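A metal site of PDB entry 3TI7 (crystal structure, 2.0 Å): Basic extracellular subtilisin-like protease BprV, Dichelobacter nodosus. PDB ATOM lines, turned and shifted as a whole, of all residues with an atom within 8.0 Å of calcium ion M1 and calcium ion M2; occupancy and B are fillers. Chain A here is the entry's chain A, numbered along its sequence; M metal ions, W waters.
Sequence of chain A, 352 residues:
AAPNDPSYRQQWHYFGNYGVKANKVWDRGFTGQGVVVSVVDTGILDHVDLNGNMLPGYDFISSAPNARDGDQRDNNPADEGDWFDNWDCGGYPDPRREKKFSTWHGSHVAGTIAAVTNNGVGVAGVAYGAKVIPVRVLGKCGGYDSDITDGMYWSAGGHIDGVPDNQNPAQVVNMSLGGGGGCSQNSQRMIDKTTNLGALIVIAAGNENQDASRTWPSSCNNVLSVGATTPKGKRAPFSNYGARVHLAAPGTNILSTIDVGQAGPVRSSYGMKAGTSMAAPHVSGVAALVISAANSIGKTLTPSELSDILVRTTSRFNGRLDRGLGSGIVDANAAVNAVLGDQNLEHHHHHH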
ATOM      1  N   TYR A  58      -5.797 -11.820   3.678  1.00  0.00           N
ATOM      2  CA  TYR A  58      -5.813 -10.651   2.797  1.00  0.00           C
ATOM      3  C   TYR A  58      -4.424 -10.048   2.652  1.00  0.00           C
ATOM      4  O   TYR A  58      -3.610 -10.093   3.576  1.00  0.00           O
ATOM      5  CB  TYR A  58      -6.813  -9.583   3.294  1.00  0.00           C
ATOM      6  CG  TYR A  58      -7.265  -8.664   2.191  1.00  0.00           C
ATOM      7  CD1 TYR A  58      -8.374  -8.983   1.390  1.00  0.00           C
ATOM      8  CD2 TYR A  58      -6.594  -7.465   1.931  1.00  0.00           C
ATOM      9  CE1 TYR A  58      -8.783  -8.138   0.356  1.00  0.00           C
ATOM     10  CE2 TYR A  58      -6.993  -6.621   0.907  1.00  0.00           C
ATOM     11  CZ  TYR A  58      -8.076  -6.957   0.119  1.00  0.00           C
ATOM     12  OH  TYR A  58      -8.465  -6.112  -0.885  1.00  0.00           O
ATOM     13  N   ASP A  59      -4.157  -9.478   1.479  1.00  0.00           N
ATOM     14  CA  ASP A  59      -2.869  -8.853   1.188  1.00  0.00           C
ATOM     15  C   ASP A  59      -3.016  -7.333   1.255  1.00  0.00           C
ATOM     16  O   ASP A  59      -3.617  -6.707   0.375  1.00  0.00           O
ATOM     17  CB  ASP A  59      -2.395  -9.294  -0.202  1.00  0.00           C
ATOM     18  CG  ASP A  59      -0.953  -8.899  -0.523  1.00  0.00           C
ATOM     19  OD1 ASP A  59      -0.453  -7.881  -0.001  1.00  0.00           O
ATOM     20  OD2 ASP A  59      -0.319  -9.609  -1.336  1.00  0.00           O
ATOM     21  N   PHE A  60      -2.445  -6.748   2.318  1.00  0.00           N
ATOM     22  CA  PHE A  60      -2.554  -5.306   2.558  1.00  0.00           C
ATOM     23  C   PHE A  60      -1.397  -4.460   2.009  1.00  0.00           C
ATOM     24  O   PHE A  60      -1.391  -3.239   2.197  1.00  0.00           O
ATOM     25  CB  PHE A  60      -2.748  -5.016   4.059  1.00  0.00           C
ATOM     26  CG  PHE A  60      -4.145  -5.286   4.544  1.00  0.00           C
ATOM     27  CD1 PHE A  60      -5.111  -4.261   4.545  1.00  0.00           C
ATOM     28  CD2 PHE A  60      -4.523  -6.561   4.968  1.00  0.00           C
ATOM     29  CE1 PHE A  60      -6.420  -4.503   4.968  1.00  0.00           C
ATOM     30  CE2 PHE A  60      -5.826  -6.813   5.404  1.00  0.00           C
ATOM     31  CZ  PHE A  60      -6.779  -5.782   5.404  1.00  0.00           C
ATOM     32  N   ILE A  61      -0.435  -5.093   1.321  1.00  0.00           N
ATOM     33  CA  ILE A  61       0.711  -4.339   0.785  1.00  0.00           C
ATOM     34  C   ILE A  61       0.252  -3.409  -0.330  1.00  0.00           C
ATOM     35  O   ILE A  61      -0.199  -3.862  -1.388  1.00  0.00           O
ATOM     36  CB  ILE A  61       1.892  -5.253   0.295  1.00  0.00           C
ATOM     37  CG1 ILE A  61       2.349  -6.220   1.389  1.00  0.00           C
ATOM     38  CG2 ILE A  61       3.077  -4.378  -0.190  1.00  0.00           C
ATOM     39  CD1 ILE A  61       3.301  -7.305   0.888  1.00  0.00           C
ATOM     40  N   SER A  62       0.366  -2.113  -0.081  1.00  0.00           N
ATOM     41  CA  SER A  62      -0.076  -1.077  -1.018  1.00  0.00           C
ATOM     42  C   SER A  62       0.880  -0.871  -2.194  1.00  0.00           C
ATOM     43  O   SER A  62       0.464  -0.479  -3.290  1.00  0.00           O
ATOM     44  CB  SER A  62      -0.323   0.237  -0.287  1.00  0.00           C
ATOM     45  OG  SER A  62      -1.368   0.104   0.667  1.00  0.00           O
ATOM     46  N   SER A  63       2.166  -1.132  -1.974  1.00  0.00           N
ATOM     47  CA  SER A  63       3.163  -1.067  -3.044  1.00  0.00           C
ATOM     48  C   SER A  63       3.160  -2.328  -3.924  1.00  0.00           C
ATOM     49  O   SER A  63       3.550  -3.406  -3.471  1.00  0.00           O
ATOM     50  CB  SER A  63       4.558  -0.840  -2.445  1.00  0.00           C
ATOM     51  OG  SER A  63       5.564  -0.943  -3.432  1.00  0.00           O
ATOM     52  N   ALA A  64       2.707  -2.183  -5.174  1.00  0.00           N
ATOM     53  CA  ALA A  64       2.748  -3.277  -6.149  1.00  0.00           C
ATOM     54  C   ALA A  64       4.166  -3.838  -6.384  1.00  0.00           C
ATOM     55  O   ALA A  64       4.318  -5.070  -6.431  1.00  0.00           O
ATOM     56  CB  ALA A  64       2.088  -2.886  -7.463  1.00  0.00           C
ATOM     57  N   PRO A  65       5.176  -2.957  -6.545  1.00  0.00           N
ATOM     58  CA  PRO A  65       6.577  -3.397  -6.635  1.00  0.00           C
ATOM     59  C   PRO A  65       7.031  -4.301  -5.474  1.00  0.00           C
ATOM     60  O   PRO A  65       7.588  -5.376  -5.697  1.00  0.00           O
ATOM     61  CB  PRO A  65       7.357  -2.085  -6.608  1.00  0.00           C
ATOM     62  CG  PRO A  65       6.452  -1.111  -7.256  1.00  0.00           C
ATOM     63  CD  PRO A  65       5.097  -1.493  -6.724  1.00  0.00           C
ATOM     64  N   ASN A  66       6.794  -3.848  -4.250  1.00  0.00           N
ATOM     65  CA  ASN A  66       7.247  -4.575  -3.082  1.00  0.00           C
ATOM     66  C   ASN A  66       6.432  -5.844  -2.788  1.00  0.00           C
ATOM     67  O   ASN A  66       6.933  -6.763  -2.162  1.00  0.00           O
ATOM     68  CB  ASN A  66       7.307  -3.640  -1.864  1.00  0.00           C
ATOM     69  CG  ASN A  66       8.352  -2.540  -2.019  1.00  0.00           C
ATOM     70  OD1 ASN A  66       9.230  -2.595  -2.879  1.00  0.00           O
ATOM     71  ND2 ASN A  66       8.269  -1.525  -1.156  1.00  0.00           N
ATOM     72  N   ALA A  67       5.200  -5.897  -3.292  1.00  0.00           N
ATOM     73  CA  ALA A  67       4.339  -7.077  -3.143  1.00  0.00           C
ATOM     74  C   ALA A  67       4.634  -8.209  -4.158  1.00  0.00           C
ATOM     75  O   ALA A  67       4.244  -9.369  -3.937  1.00  0.00           O
ATOM     76  CB  ALA A  67       2.880  -6.676  -3.196  1.00  0.00           C
ATOM     77  N   ARG A  68       5.289  -7.851  -5.260  1.00  0.00           N
ATOM     78  CA  ARG A  68       5.701  -8.778  -6.330  1.00  0.00           C
ATOM     79  C   ARG A  68       4.587  -9.627  -6.947  1.00  0.00           C
ATOM     80  O   ARG A  68       4.823 -10.746  -7.407  1.00  0.00           O
ATOM     81  CB  ARG A  68       6.869  -9.669  -5.876  1.00  0.00           C
ATOM     82  CG  ARG A  68       8.224  -8.964  -5.891  1.00  0.00           C
ATOM     83  CD  ARG A  68       9.274  -9.786  -5.172  1.00  0.00           C
ATOM     84  NE  ARG A  68      10.628  -9.299  -5.432  1.00  0.00           N
ATOM     85  CZ  ARG A  68      11.619  -9.299  -4.546  1.00  0.00           C
ATOM     86  NH1 ARG A  68      11.411  -9.751  -3.301  1.00  0.00           N
ATOM     87  NH2 ARG A  68      12.809  -8.841  -4.895  1.00  0.00           N
ATOM     88  N   ASP A  69       3.367  -9.086  -6.971  1.00  0.00           N
ATOM     89  CA  ASP A  69       2.228  -9.861  -7.462  1.00  0.00           C
ATOM     90  C   ASP A  69       1.407  -9.139  -8.534  1.00  0.00           C
ATOM     91  O   ASP A  69       0.340  -9.605  -8.919  1.00  0.00           O
ATOM     92  CB  ASP A  69       1.336 -10.275  -6.277  1.00  0.00           C
ATOM     93  CG  ASP A  69       0.874  -9.078  -5.458  1.00  0.00           C
ATOM     94  OD1 ASP A  69       1.007  -7.933  -5.925  1.00  0.00           O
ATOM     95  OD2 ASP A  69       0.353  -9.297  -4.345  1.00  0.00           O
ATOM     96  N   GLY A  70       1.910  -7.998  -9.002  1.00  0.00           N
ATOM     97  CA  GLY A  70       1.292  -7.244 -10.088  1.00  0.00           C
ATOM     98  C   GLY A  70       0.254  -6.187  -9.732  1.00  0.00           C
ATOM     99  O   GLY A  70      -0.215  -5.459 -10.621  1.00  0.00           O
ATOM    100  N   ASP A  71      -0.097  -6.075  -8.459  1.00  0.00           N
ATOM    101  CA  ASP A  71      -1.123  -5.123  -8.025  1.00  0.00           C
ATOM    102  C   ASP A  71      -0.922  -4.571  -6.602  1.00  0.00           C
ATOM    103  O   ASP A  71       0.019  -4.954  -5.908  1.00  0.00           O
ATOM    104  CB  ASP A  71      -2.526  -5.721  -8.170  1.00  0.00           C
ATOM    105  CG  ASP A  71      -2.695  -7.047  -7.440  1.00  0.00           C
ATOM    106  OD1 ASP A  71      -1.974  -7.317  -6.457  1.00  0.00           O
ATOM    107  OD2 ASP A  71      -3.556  -7.840  -7.863  1.00  0.00           O
ATOM    108  N   GLN A  72      -1.815  -3.692  -6.175  1.00  0.00           N
ATOM    109  CA  GLN A  72      -1.766  -3.157  -4.825  1.00  0.00           C
ATOM    110  C   GLN A  72      -2.514  -4.105  -3.882  1.00  0.00           C
ATOM    111  O   GLN A  72      -2.312  -5.321  -3.966  1.00  0.00           O
ATOM    112  CB  GLN A  72      -2.254  -1.707  -4.791  1.00  0.00           C
ATOM    113  CG  GLN A  72      -1.413  -0.787  -5.668  1.00  0.00           C
ATOM    114  CD  GLN A  72      -1.784   0.683  -5.519  1.00  0.00           C
ATOM    115  OE1 GLN A  72      -2.792   1.141  -6.065  1.00  0.00           O
ATOM    116  NE2 GLN A  72      -0.967   1.429  -4.794  1.00  0.00           N
ATOM    117  N   ARG A  73      -3.376  -3.611  -2.998  1.00  0.00           N
ATOM    118  CA  ARG A  73      -4.100  -4.526  -2.106  1.00  0.00           C
ATOM    119  C   ARG A  73      -4.978  -5.512  -2.871  1.00  0.00           C
ATOM    120  O   ARG A  73      -5.575  -5.168  -3.898  1.00  0.00           O
ATOM    121  CB  ARG A  73      -4.871  -3.771  -1.022  1.00  0.00           C
ATOM    122  CG  ARG A  73      -3.971  -2.973  -0.106  1.00  0.00           C
ATOM    123  CD  ARG A  73      -4.760  -2.320   1.024  1.00  0.00           C
ATOM    124  NE  ARG A  73      -3.892  -1.744   2.048  1.00  0.00           N
ATOM    125  CZ  ARG A  73      -4.321  -1.048   3.095  1.00  0.00           C
ATOM    126  NH1 ARG A  73      -5.630  -0.819   3.265  1.00  0.00           N
ATOM    127  NH2 ARG A  73      -3.456  -0.564   3.977  1.00  0.00           N
ATOM    128  N   ASP A  74      -5.037  -6.746  -2.385  1.00  0.00           N
ATOM    129  CA  ASP A  74      -5.714  -7.842  -3.078  1.00  0.00           C
ATOM    130  C   ASP A  74      -6.049  -8.964  -2.095  1.00  0.00           C
ATOM    131  O   ASP A  74      -5.561  -8.967  -0.965  1.00  0.00           O
ATOM    132  CB  ASP A  74      -4.847  -8.366  -4.233  1.00  0.00           C
ATOM    133  CG  ASP A  74      -3.580  -9.032  -3.746  1.00  0.00           C
ATOM    134  OD1 ASP A  74      -2.586  -8.335  -3.459  1.00  0.00           O
ATOM    135  OD2 ASP A  74      -3.567 -10.274  -3.652  1.00  0.00           O
ATOM    136  N   ASN A  75      -6.861  -9.924  -2.539  1.00  0.00           N
ATOM    137  CA  ASN A  75      -7.370 -10.984  -1.648  1.00  0.00           C
ATOM    138  C   ASN A  75      -6.525 -12.246  -1.555  1.00  0.00           C
ATOM    139  O   ASN A  75      -6.979 -13.266  -1.017  1.00  0.00           O
ATOM    140  CB  ASN A  75      -8.832 -11.329  -1.999  1.00  0.00           C
ATOM    141  CG  ASN A  75      -8.985 -11.924  -3.392  1.00  0.00           C
ATOM    142  OD1 ASN A  75      -8.004 -12.201  -4.077  1.00  0.00           O
ATOM    143  ND2 ASN A  75     -10.235 -12.132  -3.805  1.00  0.00           N
ATOM    144  N   ASN A  76      -5.297 -12.187  -2.074  1.00  0.00           N
ATOM    145  CA  ASN A  76      -4.397 -13.333  -2.043  1.00  0.00           C
ATOM    146  C   ASN A  76      -3.124 -13.002  -1.260  1.00  0.00           C
ATOM    147  O   ASN A  76      -2.226 -12.379  -1.806  1.00  0.00           O
ATOM    148  CB  ASN A  76      -4.047 -13.773  -3.481  1.00  0.00           C
ATOM    149  CG  ASN A  76      -3.142 -15.008  -3.531  1.00  0.00           C
ATOM    150  OD1 ASN A  76      -2.650 -15.467  -2.503  1.00  0.00           O
ATOM    151  ND2 ASN A  76      -2.950 -15.558  -4.730  1.00  0.00           N
ATOM    152  N   PRO A  77      -3.058 -13.423   0.030  1.00  0.00           N
ATOM    153  CA  PRO A  77      -1.870 -13.119   0.843  1.00  0.00           C
ATOM    154  C   PRO A  77      -0.668 -14.054   0.595  1.00  0.00           C
ATOM    155  O   PRO A  77       0.119 -14.267   1.510  1.00  0.00           O
ATOM    156  CB  PRO A  77      -2.394 -13.262   2.278  1.00  0.00           C
ATOM    157  CG  PRO A  77      -3.383 -14.397   2.172  1.00  0.00           C
ATOM    158  CD  PRO A  77      -4.068 -14.175   0.808  1.00  0.00           C
ATOM    159  N   ALA A  78      -0.549 -14.601  -0.613  1.00  0.00           N
ATOM    160  CA  ALA A  78       0.608 -15.441  -0.976  1.00  0.00           C
ATOM    161  C   ALA A  78       1.922 -14.691  -0.753  1.00  0.00           C
ATOM    162  O   ALA A  78       2.055 -13.530  -1.121  1.00  0.00           O
ATOM    163  CB  ALA A  78       0.504 -15.906  -2.434  1.00  0.00           C
ATOM    164  N   ASP A  79       2.883 -15.356  -0.102  1.00  0.00           N
ATOM    165  CA  ASP A  79       4.205 -14.768   0.100  1.00  0.00           C
ATOM    166  C   ASP A  79       4.986 -14.986  -1.181  1.00  0.00           C
ATOM    167  O   ASP A  79       5.368 -16.120  -1.497  1.00  0.00           O
ATOM    168  CB  ASP A  79       4.937 -15.393   1.295  1.00  0.00           C
ATOM    169  CG  ASP A  79       6.239 -14.654   1.666  1.00  0.00           C
ATOM    170  OD1 ASP A  79       6.672 -13.725   0.923  1.00  0.00           O
ATOM    171  OD2 ASP A  79       6.839 -14.985   2.709  1.00  0.00           O
ATOM    172  N   GLU A  80       5.208 -13.902  -1.924  1.00  0.00           N
ATOM    173  CA  GLU A  80       5.923 -13.973  -3.199  1.00  0.00           C
ATOM    174  C   GLU A  80       7.445 -14.055  -3.011  1.00  0.00           C
ATOM    175  O   GLU A  80       8.175 -14.330  -3.956  1.00  0.00           O
ATOM    176  CB  GLU A  80       5.552 -12.790  -4.102  1.00  0.00           C
ATOM    177  CG  GLU A  80       4.037 -12.528  -4.222  1.00  0.00           C
ATOM    178  CD  GLU A  80       3.314 -13.489  -5.133  1.00  0.00           C
ATOM    179  OE1 GLU A  80       3.996 -14.260  -5.859  1.00  0.00           O
ATOM    180  OE2 GLU A  80       2.054 -13.477  -5.136  1.00  0.00           O
ATOM    181  N   ARG A 136      -1.145 -10.378   4.980  1.00  0.00           N
ATOM    182  CA  ARG A 136       0.128  -9.997   4.369  1.00  0.00           C
ATOM    183  C   ARG A 136       0.320  -8.489   4.366  1.00  0.00           C
ATOM    184  O   ARG A 136      -0.470  -7.755   3.754  1.00  0.00           O
ATOM    185  CB  ARG A 136       0.269 -10.572   2.961  1.00  0.00           C
ATOM    186  CG  ARG A 136       1.671 -10.389   2.405  1.00  0.00           C
ATOM    187  CD  ARG A 136       1.756 -10.798   0.968  1.00  0.00           C
ATOM    188  NE  ARG A 136       3.144 -10.849   0.503  1.00  0.00           N
ATOM    189  CZ  ARG A 136       3.533 -10.512  -0.719  1.00  0.00           C
ATOM    190  NH1 ARG A 136       2.649 -10.058  -1.608  1.00  0.00           N
ATOM    191  NH2 ARG A 136       4.816 -10.601  -1.058  1.00  0.00           N
HETATM  192 CA    CA M   1      -1.217 -10.801  -3.246  1.00  0.00          CA
HETATM  193 CA    CA M   2      -0.887  -7.025  -4.492  1.00  0.00          CA
HETATM  194  O   HOH W   1      -0.222  -6.293  -2.655  1.00  0.00           O
HETATM  195  O   HOH W   2       0.620 -12.167  -3.118  1.00  0.00           O
HETATM  196  O   HOH W   3      -1.738 -11.717  -5.206  1.00  0.00           O
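O of Ser 62 is in hydrogen-bond range of NE2 of Gln 72, 2.8 Å away.
The backbone NH (N) of Ala 78 lies within hydrogen-bond range of the side-chain amide oxygen (OD1) of Asn 76 (3.0 Å).
The side-chain carboxylate (OD2) of Asp 59 lies close to the guanidinium group (NH1) of Arg 136, 3.0 Å away.
The backbone NH of Ile 61 is in hydrogen-bond range of the side-chain carboxylate of Asp 59 (3.1 Å).
OD2 of Asp 69 lies close to NH1 of Arg 136 (3.7 Å).
The backbone carbonyl oxygen (O) of Ala 67 sits at hydrogen-bond distance from the guanidinium group (NH1) of Arg 136 (2.9 Å).
Of the 24 residues printed, 4 come within 4 Å of calcium ion M1.
Along chain A the residues within 4 Å of calcium ion M1 span positions 59 to 76.
The nearest printed residue that does not touch calcium ion M1 is Arg 136 (4.3 Å).
Calcium ion M2 is bound by water W1 (2.1 Å), the side-chain carboxylate (OD1) of Asp 71 (2.3 Å), the backbone carbonyl oxygen (O) of Gln 72 (2.3 Å), the side-chain carboxylate (OD1) of Asp 74 (2.4 Å), the side-chain carboxylate (OD1) of Asp 69 (2.5 Å), the side-chain carboxylate (OD2) of Asp 69 (2.6 Å) and the backbone carbonyl oxygen (O) of Asp 71 (2.7 Å).
Ala 67 touches calcium ion M2 (CB to CA, 3.999 Å).
Within 4 Å of calcium ion M2: Ala 67, Asp 69, Asp 71, Gln 72 and Asp 74.
Water W2 lies within hydrogen-bond range of OE2 of Glu 80, O of Ala 78 and NH1 of Arg 136.
Water W1 lies within hydrogen-bond range of the backbone carbonyl oxygen (O) of Ile 61 (2.7 Å) and the side-chain carboxylate (OD1) of Asp 59 (3.1 Å).
Calcium ion M1 is bound by water W3 (2.2 Å), water W2 (2.3 Å), O of Asn 76 (2.4 Å), OD2 of Asp 59 (2.4 Å), OD2 of Asp 69 (2.4 Å), OD2 of Asp 74 (2.4 Å) and OD1 of Asp 74 (2.8 Å).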
